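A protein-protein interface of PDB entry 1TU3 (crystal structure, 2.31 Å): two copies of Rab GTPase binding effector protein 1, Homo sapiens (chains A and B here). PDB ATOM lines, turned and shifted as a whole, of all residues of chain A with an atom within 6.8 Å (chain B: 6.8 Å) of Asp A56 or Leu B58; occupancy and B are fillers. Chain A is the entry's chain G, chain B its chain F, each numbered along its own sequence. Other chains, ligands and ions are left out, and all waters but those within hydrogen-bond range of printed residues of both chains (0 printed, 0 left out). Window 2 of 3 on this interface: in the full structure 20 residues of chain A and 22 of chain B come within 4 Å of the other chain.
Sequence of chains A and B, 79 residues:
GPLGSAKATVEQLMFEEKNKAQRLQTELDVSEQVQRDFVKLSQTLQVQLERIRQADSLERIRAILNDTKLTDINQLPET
Hydrophobic or aromatic side chains of chain B within 4 Å of the printed part of chain A: Leu B58 and Ile B61.
Of the 11 printed residues of chain A, 3 touch a printed residue of chain B.
Hydrophobic or aromatic side chains of chain A within 4 Å of the printed part of chain B: Leu A58 and Ile A61.
Among the printed residues, 6 pairs touch across the chains.
Among the printed residues, no Asp or Glu carboxylate lies within 4 Å of a Lys or Arg side-chain nitrogen of the other chain.
Asp A56 touches one residue of chain B.
Leu B58 touches three residues of chain A.
Of the printed residues of chain B, Ile A61 touches Leu B58 and Ile B61.
Of the printed residues of chain B, Leu A58 touches Asp B56, Ser B57 and Leu B58.
Printed residues of chain A within 4 Å of Ser B57: Leu A58.
Printed residues of chain A within 4 Å of Asp B56: Leu A58 (3.9 Å).
Ala B55 touches none of the printed residues of chain A.
Glu B59 touches none of the printed residues of chain A.
The nearest printed residue of chain B that does not touch Asp A56 is Arg B62 (8.2 Å).
The nearest printed residue of chain A that does not touch Ile B61 is Leu A58 (4.02 Å).
Asp A56 touches Leu B58, and with the chains exchanged Leu A58 touches Asp B56.
Leu A58 touches Ser B57, but with the chains exchanged Ser A57 does not touch Leu B58 (4.2 Å).
Leu A58 touches its own counterpart, Leu B58.
Ile B61 touches its own counterpart, Ile A61.
Asp A56 touches Leu B58 (O to CD1, 3.7 Å).
O of Asp B56 touches CD2 of Leu A58, at 3.9 Å.
Leu A58 touches Ser B57.
Leu A58 touches Leu B58.
CD2 of Leu B58 touches CD1 of Ile A61 (3.6 Å).
CD1 of Ile B61 touches CD1 of Ile A61, 3.2 Å away.
The side-chain carboxylate (OD1) of Asp B56 lies within salt-bridge range of the guanidinium group (NH1) of Arg B60 (3.5 Å).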
ATOM      1  N   ARG A  51       2.125 -26.652 -35.458  1.00  0.00           N
ATOM      2  CA  ARG A  51       2.716 -27.984 -35.425  1.00  0.00           C
ATOM      3  C   ARG A  51       3.254 -28.310 -34.028  1.00  0.00           C
ATOM      4  O   ARG A  51       2.905 -29.330 -33.449  1.00  0.00           O
ATOM      5  CB  ARG A  51       3.852 -28.100 -36.425  1.00  0.00           C
ATOM      6  CG  ARG A  51       3.422 -28.336 -37.851  1.00  0.00           C
ATOM      7  CD  ARG A  51       4.592 -28.919 -38.650  1.00  0.00           C
ATOM      8  NE  ARG A  51       5.521 -27.894 -39.110  1.00  0.00           N
ATOM      9  CZ  ARG A  51       6.768 -28.135 -39.507  1.00  0.00           C
ATOM     10  NH1 ARG A  51       7.237 -29.377 -39.490  1.00  0.00           N
ATOM     11  NH2 ARG A  51       7.538 -27.135 -39.934  1.00  0.00           N
ATOM     12  N   ILE A  52       4.097 -27.438 -33.488  1.00  0.00           N
ATOM     13  CA  ILE A  52       4.632 -27.653 -32.150  1.00  0.00           C
ATOM     14  C   ILE A  52       3.529 -27.822 -31.104  1.00  0.00           C
ATOM     15  O   ILE A  52       3.633 -28.662 -30.218  1.00  0.00           O
ATOM     16  CB  ILE A  52       5.556 -26.490 -31.740  1.00  0.00           C
ATOM     17  CG1 ILE A  52       6.892 -26.630 -32.484  1.00  0.00           C
ATOM     18  CG2 ILE A  52       5.757 -26.478 -30.227  1.00  0.00           C
ATOM     19  CD1 ILE A  52       7.765 -25.422 -32.349  1.00  0.00           C
ATOM     20  N   ARG A  53       2.474 -27.029 -31.220  1.00  0.00           N
ATOM     21  CA  ARG A  53       1.331 -27.139 -30.329  1.00  0.00           C
ATOM     22  C   ARG A  53       0.692 -28.518 -30.428  1.00  0.00           C
ATOM     23  O   ARG A  53       0.036 -28.982 -29.501  1.00  0.00           O
ATOM     24  CB  ARG A  53       0.285 -26.082 -30.698  1.00  0.00           C
ATOM     25  CG  ARG A  53      -0.290 -25.341 -29.504  1.00  0.00           C
ATOM     26  CD  ARG A  53      -1.781 -25.496 -29.414  1.00  0.00           C
ATOM     27  NE  ARG A  53      -2.473 -25.096 -30.634  1.00  0.00           N
ATOM     28  CZ  ARG A  53      -3.791 -25.200 -30.808  1.00  0.00           C
ATOM     29  NH1 ARG A  53      -4.554 -25.686 -29.837  1.00  0.00           N
ATOM     30  NH2 ARG A  53      -4.353 -24.833 -31.955  1.00  0.00           N
ATOM     31  N   GLN A  54       0.874 -29.168 -31.568  1.00  0.00           N
ATOM     32  CA  GLN A  54       0.270 -30.464 -31.797  1.00  0.00           C
ATOM     33  C   GLN A  54       1.250 -31.596 -31.511  1.00  0.00           C
ATOM     34  O   GLN A  54       0.879 -32.767 -31.548  1.00  0.00           O
ATOM     35  CB  GLN A  54      -0.221 -30.568 -33.246  1.00  0.00           C
ATOM     36  CG  GLN A  54      -1.297 -29.555 -33.627  1.00  0.00           C
ATOM     37  CD  GLN A  54      -2.547 -29.686 -32.784  1.00  0.00           C
ATOM     38  OE1 GLN A  54      -3.018 -30.794 -32.529  1.00  0.00           O
ATOM     39  NE2 GLN A  54      -3.096 -28.562 -32.353  1.00  0.00           N
ATOM     40  N   ALA A  55       2.504 -31.265 -31.226  1.00  0.00           N
ATOM     41  CA  ALA A  55       3.504 -32.310 -31.090  1.00  0.00           C
ATOM     42  C   ALA A  55       3.227 -33.140 -29.842  1.00  0.00           C
ATOM     43  O   ALA A  55       2.857 -32.608 -28.795  1.00  0.00           O
ATOM     44  CB  ALA A  55       4.908 -31.716 -31.028  1.00  0.00           C
ATOM     45  N   ASP A  56       3.403 -34.449 -29.970  1.00  0.00           N
ATOM     46  CA  ASP A  56       3.199 -35.368 -28.862  1.00  0.00           C
ATOM     47  C   ASP A  56       4.382 -35.372 -27.897  1.00  0.00           C
ATOM     48  O   ASP A  56       4.224 -35.116 -26.701  1.00  0.00           O
ATOM     49  CB  ASP A  56       2.982 -36.777 -29.403  1.00  0.00           C
ATOM     50  CG  ASP A  56       3.008 -37.823 -28.315  1.00  0.00           C
ATOM     51  OD1 ASP A  56       2.159 -37.744 -27.401  1.00  0.00           O
ATOM     52  OD2 ASP A  56       3.880 -38.720 -28.374  1.00  0.00           O
ATOM     53  N   SER A  57       5.567 -35.659 -28.424  1.00  0.00           N
ATOM     54  CA  SER A  57       6.750 -35.796 -27.593  1.00  0.00           C
ATOM     55  C   SER A  57       7.670 -34.588 -27.729  1.00  0.00           C
ATOM     56  O   SER A  57       7.543 -33.805 -28.675  1.00  0.00           O
ATOM     57  CB  SER A  57       7.508 -37.064 -27.983  1.00  0.00           C
ATOM     58  OG  SER A  57       7.908 -37.009 -29.340  1.00  0.00           O
ATOM     59  N   LEU A  58       8.597 -34.444 -26.785  1.00  0.00           N
ATOM     60  CA  LEU A  58       9.576 -33.366 -26.830  1.00  0.00           C
ATOM     61  C   LEU A  58      10.556 -33.581 -27.988  1.00  0.00           C
ATOM     62  O   LEU A  58      11.132 -32.631 -28.527  1.00  0.00           O
ATOM     63  CB  LEU A  58      10.351 -33.310 -25.513  1.00  0.00           C
ATOM     64  CG  LEU A  58      10.880 -31.937 -25.103  1.00  0.00           C
ATOM     65  CD1 LEU A  58       9.832 -31.224 -24.252  1.00  0.00           C
ATOM     66  CD2 LEU A  58      12.164 -32.094 -24.332  1.00  0.00           C
ATOM     67  N   GLU A  59      10.738 -34.839 -28.370  1.00  0.00           N
ATOM     68  CA  GLU A  59      11.607 -35.166 -29.489  1.00  0.00           C
ATOM     69  C   GLU A  59      10.946 -34.774 -30.812  1.00  0.00           C
ATOM     70  O   GLU A  59      11.629 -34.434 -31.782  1.00  0.00           O
ATOM     71  CB  GLU A  59      11.921 -36.661 -29.483  1.00  0.00           C
ATOM     72  CG  GLU A  59      13.051 -37.065 -30.401  1.00  0.00           C
ATOM     73  CD  GLU A  59      13.303 -38.558 -30.364  1.00  0.00           C
ATOM     74  OE1 GLU A  59      13.480 -39.099 -29.250  1.00  0.00           O
ATOM     75  OE2 GLU A  59      13.323 -39.190 -31.447  1.00  0.00           O
ATOM     76  N   ARG A  60       9.616 -34.826 -30.846  1.00  0.00           N
ATOM     77  CA  ARG A  60       8.873 -34.343 -31.999  1.00  0.00           C
ATOM     78  C   ARG A  60       9.078 -32.833 -32.181  1.00  0.00           C
ATOM     79  O   ARG A  60       9.122 -32.324 -33.298  1.00  0.00           O
ATOM     80  CB  ARG A  60       7.382 -34.627 -31.839  1.00  0.00           C
ATOM     81  CG  ARG A  60       6.538 -34.222 -33.068  1.00  0.00           C
ATOM     82  CD  ARG A  60       6.665 -35.209 -34.230  1.00  0.00           C
ATOM     83  NE  ARG A  60       8.051 -35.619 -34.469  1.00  0.00           N
ATOM     84  CZ  ARG A  60       8.416 -36.790 -34.996  1.00  0.00           C
ATOM     85  NH1 ARG A  60       7.497 -37.688 -35.356  1.00  0.00           N
ATOM     86  NH2 ARG A  60       9.708 -37.079 -35.135  1.00  0.00           N
ATOM     87  N   ILE A  61       9.200 -32.116 -31.076  1.00  0.00           N
ATOM     88  CA  ILE A  61       9.297 -30.675 -31.152  1.00  0.00           C
ATOM     89  C   ILE A  61      10.643 -30.247 -31.730  1.00  0.00           C
ATOM     90  O   ILE A  61      10.704 -29.310 -32.541  1.00  0.00           O
ATOM     91  CB  ILE A  61       9.075 -30.064 -29.777  1.00  0.00           C
ATOM     92  CG1 ILE A  61       7.643 -30.360 -29.340  1.00  0.00           C
ATOM     93  CG2 ILE A  61       9.307 -28.569 -29.818  1.00  0.00           C
ATOM     94  CD1 ILE A  61       7.294 -29.879 -27.956  1.00  0.00           C
ATOM     95  N   ALA B  55      13.259 -24.191 -24.114  1.00  0.00           N
ATOM     96  CA  ALA B  55      12.408 -24.851 -23.125  1.00  0.00           C
ATOM     97  C   ALA B  55      12.936 -26.234 -22.744  1.00  0.00           C
ATOM     98  O   ALA B  55      13.411 -26.999 -23.587  1.00  0.00           O
ATOM     99  CB  ALA B  55      10.977 -24.964 -23.644  1.00  0.00           C
ATOM    100  N   ASP B  56      12.832 -26.546 -21.459  1.00  0.00           N
ATOM    101  CA  ASP B  56      13.384 -27.774 -20.899  1.00  0.00           C
ATOM    102  C   ASP B  56      12.411 -28.956 -20.938  1.00  0.00           C
ATOM    103  O   ASP B  56      12.838 -30.106 -21.071  1.00  0.00           O
ATOM    104  CB  ASP B  56      13.813 -27.509 -19.458  1.00  0.00           C
ATOM    105  CG  ASP B  56      12.773 -26.714 -18.689  1.00  0.00           C
ATOM    106  OD1 ASP B  56      12.509 -25.548 -19.069  1.00  0.00           O
ATOM    107  OD2 ASP B  56      12.214 -27.260 -17.714  1.00  0.00           O
ATOM    108  N   SER B  57      11.114 -28.672 -20.821  1.00  0.00           N
ATOM    109  CA  SER B  57      10.097 -29.724 -20.803  1.00  0.00           C
ATOM    110  C   SER B  57       8.772 -29.270 -21.407  1.00  0.00           C
ATOM    111  O   SER B  57       8.522 -28.075 -21.555  1.00  0.00           O
ATOM    112  CB  SER B  57       9.858 -30.201 -19.366  1.00  0.00           C
ATOM    113  OG  SER B  57       8.877 -31.229 -19.318  1.00  0.00           O
ATOM    114  N   LEU B  58       7.924 -30.241 -21.745  1.00  0.00           N
ATOM    115  CA  LEU B  58       6.619 -29.964 -22.339  1.00  0.00           C
ATOM    116  C   LEU B  58       5.797 -29.023 -21.471  1.00  0.00           C
ATOM    117  O   LEU B  58       4.888 -28.355 -21.960  1.00  0.00           O
ATOM    118  CB  LEU B  58       5.844 -31.266 -22.561  1.00  0.00           C
ATOM    119  CG  LEU B  58       6.414 -32.276 -23.563  1.00  0.00           C
ATOM    120  CD1 LEU B  58       5.536 -33.513 -23.597  1.00  0.00           C
ATOM    121  CD2 LEU B  58       6.490 -31.655 -24.937  1.00  0.00           C
ATOM    122  N   GLU B  59       6.121 -28.975 -20.182  1.00  0.00           N
ATOM    123  CA  GLU B  59       5.478 -28.037 -19.268  1.00  0.00           C
ATOM    124  C   GLU B  59       5.713 -26.612 -19.749  1.00  0.00           C
ATOM    125  O   GLU B  59       4.791 -25.949 -20.231  1.00  0.00           O
ATOM    126  CB  GLU B  59       6.049 -28.195 -17.852  1.00  0.00           C
ATOM    127  CG  GLU B  59       5.672 -29.492 -17.151  1.00  0.00           C
ATOM    128  CD  GLU B  59       6.355 -29.650 -15.801  1.00  0.00           C
ATOM    129  OE1 GLU B  59       7.599 -29.761 -15.779  1.00  0.00           O
ATOM    130  OE2 GLU B  59       5.656 -29.660 -14.765  1.00  0.00           O
ATOM    131  N   ARG B  60       6.957 -26.159 -19.612  1.00  0.00           N
ATOM    132  CA  ARG B  60       7.338 -24.807 -20.003  1.00  0.00           C
ATOM    133  C   ARG B  60       6.789 -24.505 -21.391  1.00  0.00           C
ATOM    134  O   ARG B  60       6.285 -23.413 -21.638  1.00  0.00           O
ATOM    135  CB  ARG B  60       8.867 -24.670 -19.997  1.00  0.00           C
ATOM    136  CG  ARG B  60       9.414 -23.652 -18.991  1.00  0.00           C
ATOM    137  CD  ARG B  60       9.316 -22.220 -19.515  1.00  0.00           C
ATOM    138  NE  ARG B  60      10.295 -21.959 -20.571  1.00  0.00           N
ATOM    139  CZ  ARG B  60      11.610 -21.878 -20.375  1.00  0.00           C
ATOM    140  NH1 ARG B  60      12.111 -22.032 -19.155  1.00  0.00           N
ATOM    141  NH2 ARG B  60      12.427 -21.654 -21.400  1.00  0.00           N
ATOM    142  N   ILE B  61       6.868 -25.488 -22.281  1.00  0.00           N
ATOM    143  CA  ILE B  61       6.500 -25.276 -23.671  1.00  0.00           C
ATOM    144  C   ILE B  61       5.047 -24.872 -23.822  1.00  0.00           C
ATOM    145  O   ILE B  61       4.738 -23.851 -24.425  1.00  0.00           O
ATOM    146  CB  ILE B  61       6.753 -26.529 -24.533  1.00  0.00           C
ATOM    147  CG1 ILE B  61       8.236 -26.635 -24.885  1.00  0.00           C
ATOM    148  CG2 ILE B  61       5.924 -26.468 -25.807  1.00  0.00           C
ATOM    149  CD1 ILE B  61       8.551 -27.760 -25.840  1.00  0.00           C
ATOM    150  N   ARG B  62       4.151 -25.686 -23.287  1.00  0.00           N
ATOM    151  CA  ARG B  62       2.730 -25.380 -23.349  1.00  0.00           C
ATOM    152  C   ARG B  62       2.414 -24.079 -22.598  1.00  0.00           C
ATOM    153  O   ARG B  62       1.451 -23.383 -22.916  1.00  0.00           O
ATOM    154  CB  ARG B  62       1.929 -26.536 -22.766  1.00  0.00           C
ATOM    155  CG  ARG B  62       2.027 -26.653 -21.254  1.00  0.00           C
ATOM    156  CD  ARG B  62       1.550 -28.021 -20.809  1.00  0.00           C
ATOM    157  NE  ARG B  62       0.356 -28.428 -21.543  1.00  0.00           N
ATOM    158  CZ  ARG B  62      -0.111 -29.671 -21.578  1.00  0.00           C
ATOM    159  NH1 ARG B  62       0.514 -30.639 -20.918  1.00  0.00           N
ATOM    160  NH2 ARG B  62      -1.202 -29.946 -22.282  1.00  0.00           N
ATOM    161  N   ALA B  63       3.230 -23.749 -21.603  1.00  0.00           N
ATOM    162  CA  ALA B  63       3.096 -22.467 -20.913  1.00  0.00           C
ATOM    163  C   ALA B  63       3.408 -21.295 -21.853  1.00  0.00           C
ATOM    164  O   ALA B  63       2.712 -20.280 -21.843  1.00  0.00           O
ATOM    165  CB  ALA B  63       4.021 -22.429 -19.702  1.00  0.00           C
